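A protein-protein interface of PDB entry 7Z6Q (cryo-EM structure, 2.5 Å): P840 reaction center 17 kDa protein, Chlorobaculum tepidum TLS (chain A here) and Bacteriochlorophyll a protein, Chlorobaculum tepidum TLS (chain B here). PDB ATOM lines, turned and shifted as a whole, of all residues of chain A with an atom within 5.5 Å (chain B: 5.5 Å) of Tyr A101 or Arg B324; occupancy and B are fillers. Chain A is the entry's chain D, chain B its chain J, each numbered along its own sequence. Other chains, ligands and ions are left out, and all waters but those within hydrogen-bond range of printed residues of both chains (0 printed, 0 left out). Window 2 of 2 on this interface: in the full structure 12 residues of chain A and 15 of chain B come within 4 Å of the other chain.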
ATOM      1  N   MET A  97       2.965 -20.478  -5.161  1.00  0.00           N
ATOM      2  CA  MET A  97       3.016 -18.998  -5.009  1.00  0.00           C
ATOM      3  C   MET A  97       3.330 -18.624  -3.556  1.00  0.00           C
ATOM      4  O   MET A  97       4.164 -17.721  -3.348  1.00  0.00           O
ATOM      5  CB  MET A  97       1.683 -18.363  -5.419  1.00  0.00           C
ATOM      6  CG  MET A  97       1.659 -16.853  -5.263  1.00  0.00           C
ATOM      7  SD  MET A  97       2.783 -16.017  -6.412  1.00  0.00           S
ATOM      8  CE  MET A  97       2.526 -14.309  -5.940  1.00  0.00           C
ATOM      9  N   GLU A  98       2.666 -19.284  -2.600  1.00  0.00           N
ATOM     10  CA  GLU A  98       2.886 -19.013  -1.154  1.00  0.00           C
ATOM     11  C   GLU A  98       4.370 -19.220  -0.833  1.00  0.00           C
ATOM     12  O   GLU A  98       4.951 -18.363  -0.140  1.00  0.00           O
ATOM     13  CB  GLU A  98       2.005 -19.927  -0.300  1.00  0.00           C
ATOM     14  CG  GLU A  98       1.675 -19.346   1.064  1.00  0.00           C
ATOM     15  CD  GLU A  98       0.900 -18.039   1.025  1.00  0.00           C
ATOM     16  OE1 GLU A  98       0.805 -17.443  -0.066  1.00  0.00           O
ATOM     17  OE2 GLU A  98       0.395 -17.622   2.085  1.00  0.00           O
ATOM     18  N   ASN A  99       4.946 -20.321  -1.327  1.00  0.00           N
ATOM     19  CA  ASN A  99       6.383 -20.628  -1.098  1.00  0.00           C
ATOM     20  C   ASN A  99       7.239 -19.534  -1.747  1.00  0.00           C
ATOM     21  O   ASN A  99       8.222 -19.097  -1.124  1.00  0.00           O
ATOM     22  CB  ASN A  99       6.744 -22.027  -1.606  1.00  0.00           C
ATOM     23  CG  ASN A  99       6.541 -23.098  -0.557  1.00  0.00           C
ATOM     24  OD1 ASN A  99       6.868 -22.897   0.610  1.00  0.00           O
ATOM     25  ND2 ASN A  99       5.999 -24.237  -0.955  1.00  0.00           N
ATOM     26  N   ARG A 100       6.822 -18.976  -2.888  1.00  0.00           N
ATOM     27  CA  ARG A 100       7.640 -17.927  -3.573  1.00  0.00           C
ATOM     28  C   ARG A 100       7.945 -16.724  -2.659  1.00  0.00           C
ATOM     29  O   ARG A 100       9.126 -16.351  -2.573  1.00  0.00           O
ATOM     30  CB  ARG A 100       7.045 -17.501  -4.919  1.00  0.00           C
ATOM     31  CG  ARG A 100       8.102 -17.130  -5.950  1.00  0.00           C
ATOM     32  CD  ARG A 100       7.578 -16.608  -7.273  1.00  0.00           C
ATOM     33  NE  ARG A 100       6.532 -15.613  -7.098  1.00  0.00           N
ATOM     34  CZ  ARG A 100       6.614 -14.353  -7.497  1.00  0.00           C
ATOM     35  NH1 ARG A 100       7.744 -13.886  -7.994  1.00  0.00           N
ATOM     36  NH2 ARG A 100       5.564 -13.565  -7.398  1.00  0.00           N
ATOM     37  N   TYR A 101       6.940 -16.103  -2.033  1.00  0.00           N
ATOM     38  CA  TYR A 101       7.242 -14.949  -1.140  1.00  0.00           C
ATOM     39  C   TYR A 101       6.886 -15.260   0.322  1.00  0.00           C
ATOM     40  O   TYR A 101       6.483 -14.326   1.042  1.00  0.00           O
ATOM     41  CB  TYR A 101       6.513 -13.689  -1.614  1.00  0.00           C
ATOM     42  CG  TYR A 101       5.020 -13.710  -1.393  1.00  0.00           C
ATOM     43  CD1 TYR A 101       4.432 -12.961  -0.388  1.00  0.00           C
ATOM     44  CD2 TYR A 101       4.194 -14.486  -2.187  1.00  0.00           C
ATOM     45  CE1 TYR A 101       3.062 -12.975  -0.186  1.00  0.00           C
ATOM     46  CE2 TYR A 101       2.825 -14.514  -1.995  1.00  0.00           C
ATOM     47  CZ  TYR A 101       2.256 -13.755  -0.991  1.00  0.00           C
ATOM     48  OH  TYR A 101       0.905 -13.786  -0.806  1.00  0.00           O
ATOM     49  N   ARG A 115      -8.641 -18.932  -1.337  1.00  0.00           N
ATOM     50  CA  ARG A 115      -8.747 -17.592  -1.960  1.00  0.00           C
ATOM     51  C   ARG A 115     -10.098 -17.480  -2.673  1.00  0.00           C
ATOM     52  O   ARG A 115     -10.763 -18.495  -2.838  1.00  0.00           O
ATOM     53  CB  ARG A 115      -7.607 -17.307  -2.948  1.00  0.00           C
ATOM     54  CG  ARG A 115      -6.311 -18.082  -2.742  1.00  0.00           C
ATOM     55  CD  ARG A 115      -5.463 -17.464  -1.648  1.00  0.00           C
ATOM     56  NE  ARG A 115      -4.057 -17.843  -1.672  1.00  0.00           N
ATOM     57  CZ  ARG A 115      -3.066 -16.998  -1.417  1.00  0.00           C
ATOM     58  NH1 ARG A 115      -3.338 -15.735  -1.130  1.00  0.00           N
ATOM     59  NH2 ARG A 115      -1.813 -17.408  -1.457  1.00  0.00           N
ATOM     60  N   GLY B 282      -1.151 -17.221  -6.831  1.00  0.00           N
ATOM     61  CA  GLY B 282      -1.432 -17.190  -5.404  1.00  0.00           C
ATOM     62  C   GLY B 282      -2.282 -16.019  -4.964  1.00  0.00           C
ATOM     63  O   GLY B 282      -2.091 -15.500  -3.857  1.00  0.00           O
ATOM     64  N   LEU B 284      -2.176 -13.074  -5.980  1.00  0.00           N
ATOM     65  CA  LEU B 284      -1.423 -11.790  -5.991  1.00  0.00           C
ATOM     66  C   LEU B 284      -1.398 -11.163  -7.388  1.00  0.00           C
ATOM     67  O   LEU B 284      -1.205 -11.900  -8.375  1.00  0.00           O
ATOM     68  CB  LEU B 284       0.000 -12.050  -5.483  1.00  0.00           C
ATOM     69  CG  LEU B 284       0.170 -12.022  -3.965  1.00  0.00           C
ATOM     70  CD1 LEU B 284      -0.653 -13.121  -3.308  1.00  0.00           C
ATOM     71  CD2 LEU B 284       1.635 -12.152  -3.579  1.00  0.00           C
ATOM     72  N   LYS B 322      -2.732  -3.645  -0.698  1.00  0.00           N
ATOM     73  CA  LYS B 322      -1.431  -3.303  -0.120  1.00  0.00           C
ATOM     74  C   LYS B 322      -0.328  -4.182  -0.731  1.00  0.00           C
ATOM     75  O   LYS B 322      -0.545  -5.381  -0.810  1.00  0.00           O
ATOM     76  CB  LYS B 322      -1.569  -3.472   1.402  1.00  0.00           C
ATOM     77  CG  LYS B 322      -2.477  -2.490   2.138  1.00  0.00           C
ATOM     78  CD  LYS B 322      -2.546  -2.667   3.648  1.00  0.00           C
ATOM     79  CE  LYS B 322      -3.239  -3.963   4.023  1.00  0.00           C
ATOM     80  NZ  LYS B 322      -4.659  -4.075   3.616  1.00  0.00           N
ATOM     81  N   ILE B 323       0.854  -3.600  -0.976  1.00  0.00           N
ATOM     82  CA  ILE B 323       2.031  -4.327  -1.542  1.00  0.00           C
ATOM     83  C   ILE B 323       2.405  -5.512  -0.636  1.00  0.00           C
ATOM     84  O   ILE B 323       2.473  -5.313   0.591  1.00  0.00           O
ATOM     85  CB  ILE B 323       3.204  -3.342  -1.710  1.00  0.00           C
ATOM     86  CG1 ILE B 323       3.077  -2.526  -2.999  1.00  0.00           C
ATOM     87  CG2 ILE B 323       4.541  -4.061  -1.615  1.00  0.00           C
ATOM     88  CD1 ILE B 323       4.061  -1.392  -3.114  1.00  0.00           C
ATOM     89  N   ARG B 324       2.676  -6.665  -1.263  1.00  0.00           N
ATOM     90  CA  ARG B 324       3.193  -7.861  -0.558  1.00  0.00           C
ATOM     91  C   ARG B 324       4.726  -7.829  -0.643  1.00  0.00           C
ATOM     92  O   ARG B 324       5.350  -8.293   0.338  1.00  0.00           O
ATOM     93  CB  ARG B 324       2.634  -9.144  -1.180  1.00  0.00           C
ATOM     94  CG  ARG B 324       1.119  -9.268  -1.094  1.00  0.00           C
ATOM     95  CD  ARG B 324       0.605  -9.458   0.320  1.00  0.00           C
ATOM     96  NE  ARG B 324      -0.846  -9.573   0.357  1.00  0.00           N
ATOM     97  CZ  ARG B 324      -1.524 -10.700   0.168  1.00  0.00           C
ATOM     98  NH1 ARG B 324      -2.845 -10.696   0.228  1.00  0.00           N
ATOM     99  NH2 ARG B 324      -0.881 -11.826  -0.082  1.00  0.00           N
ATOM    100  N   TYR B 325       5.287  -7.248  -1.727  1.00  0.00           N
ATOM    101  CA  TYR B 325       6.704  -7.191  -1.953  1.00  0.00           C
ATOM    102  C   TYR B 325       7.076  -6.288  -3.105  1.00  0.00           C
ATOM    103  O   TYR B 325       6.377  -6.273  -4.093  1.00  0.00           O
ATOM    104  CB  TYR B 325       7.164  -8.629  -2.271  1.00  0.00           C
ATOM    105  CG  TYR B 325       8.453  -8.757  -3.033  1.00  0.00           C
ATOM    106  CD1 TYR B 325       9.658  -8.855  -2.369  1.00  0.00           C
ATOM    107  CD2 TYR B 325       8.462  -8.797  -4.412  1.00  0.00           C
ATOM    108  CE1 TYR B 325      10.838  -8.981  -3.056  1.00  0.00           C
ATOM    109  CE2 TYR B 325       9.640  -8.922  -5.105  1.00  0.00           C
ATOM    110  CZ  TYR B 325      10.824  -9.012  -4.420  1.00  0.00           C
ATOM    111  OH  TYR B 325      12.001  -9.139  -5.113  1.00  0.00           O
ATOM    112  N   ALA B 326       8.168  -5.536  -2.970  1.00  0.00           N
ATOM    113  CA  ALA B 326       8.720  -4.712  -4.070  1.00  0.00           C
ATOM    114  C   ALA B 326      10.240  -4.750  -3.884  1.00  0.00           C
ATOM    115  O   ALA B 326      10.687  -4.527  -2.760  1.00  0.00           O
ATOM    116  CB  ALA B 326       8.207  -3.296  -4.112  1.00  0.00           C
ATOM    117  N   LEU B 363       4.339  -6.571  -6.048  1.00  0.00           N
ATOM    118  CA  LEU B 363       3.219  -7.530  -5.894  1.00  0.00           C
ATOM    119  C   LEU B 363       2.232  -6.897  -4.917  1.00  0.00           C
ATOM    120  O   LEU B 363       2.627  -6.651  -3.773  1.00  0.00           O
ATOM    121  CB  LEU B 363       3.754  -8.835  -5.300  1.00  0.00           C
ATOM    122  CG  LEU B 363       4.735  -9.622  -6.164  1.00  0.00           C
ATOM    123  CD1 LEU B 363       5.155 -10.907  -5.470  1.00  0.00           C
ATOM    124  CD2 LEU B 363       4.141  -9.919  -7.527  1.00  0.00           C
ATOM    125  N   TYR B 364       0.997  -6.650  -5.368  1.00  0.00           N
ATOM    126  CA  TYR B 364      -0.047  -6.033  -4.507  1.00  0.00           C
ATOM    127  C   TYR B 364      -1.272  -6.953  -4.450  1.00  0.00           C
ATOM    128  O   TYR B 364      -1.846  -7.260  -5.513  1.00  0.00           O
ATOM    129  CB  TYR B 364      -0.420  -4.644  -5.032  1.00  0.00           C
ATOM    130  CG  TYR B 364      -1.097  -4.642  -6.380  1.00  0.00           C
ATOM    131  CD1 TYR B 364      -0.358  -4.580  -7.551  1.00  0.00           C
ATOM    132  CD2 TYR B 364      -2.476  -4.701  -6.487  1.00  0.00           C
ATOM    133  CE1 TYR B 364      -0.972  -4.577  -8.792  1.00  0.00           C
ATOM    134  CE2 TYR B 364      -3.105  -4.699  -7.722  1.00  0.00           C
ATOM    135  CZ  TYR B 364      -2.351  -4.637  -8.879  1.00  0.00           C
ATOM    136  OH  TYR B 364      -2.964  -4.635 -10.099  1.00  0.00           O
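The side-chain hydroxyl (OH) of Tyr A101 is in hydrogen-bond range of the guanidinium group (NH2) of Arg B324 (2.7 Å).
The guanidinium group of Arg A115 lies within hydrogen-bond range of the backbone carbonyl oxygen of Gly B282 (3.0 Å).
The guanidinium group (NH2) of Arg A115 lies within salt-bridge range of the side-chain carboxylate (OE1) of Glu A98, at 3.0 Å.
O of Leu B363 is in hydrogen-bond range of N of Arg B324, at 2.5 Å.
O of Tyr B325 is in hydrogen-bond range of N of Leu B363, at 2.8 Å.
Of chain B, only Leu B284 (3.0 Å) and Arg B324 (2.7 Å) come within 4 Å of Tyr A101.
Of chain A, only Tyr A101 (2.7 Å) comes within 4 Å of Arg B324.
Of the printed residues of chain A, Leu B284 touches Met A97 and Tyr A101.
Printed residues of chain A within 4 Å of Leu B363: Arg A100 (3.3 Å).
Of the printed residues of chain B, Arg A100 touches Leu B363.
Of the printed residues of chain B, Met A97 touches Gly B282 and Leu B284.
Among the printed residues, pairs that only touch across the chains: Met A97 with Gly B282 (3.1 Å), Met A97 with Leu B284 (3.3 Å), Arg A100 with Leu B363 (3.3 Å) and Tyr A101 with Leu B284 (3.0 Å).
Hydrophobic or aromatic side chains of chain A within 4 Å of the printed part of chain B: Met A97 and Tyr A101.
Printed residues of chain B that touch a printed residue of chain A: Gly B282, Leu B284, Arg B324 and Leu B363.
Hydrophobic or aromatic side chains of chain B that line the printed part of chain A: Leu B284 and Leu B363.
Among the printed residues, 6 pairs touch across the chains.
Among the printed residues, no Asp or Glu carboxylate lies within 4 Å of a Lys or Arg side-chain nitrogen of the other chain.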
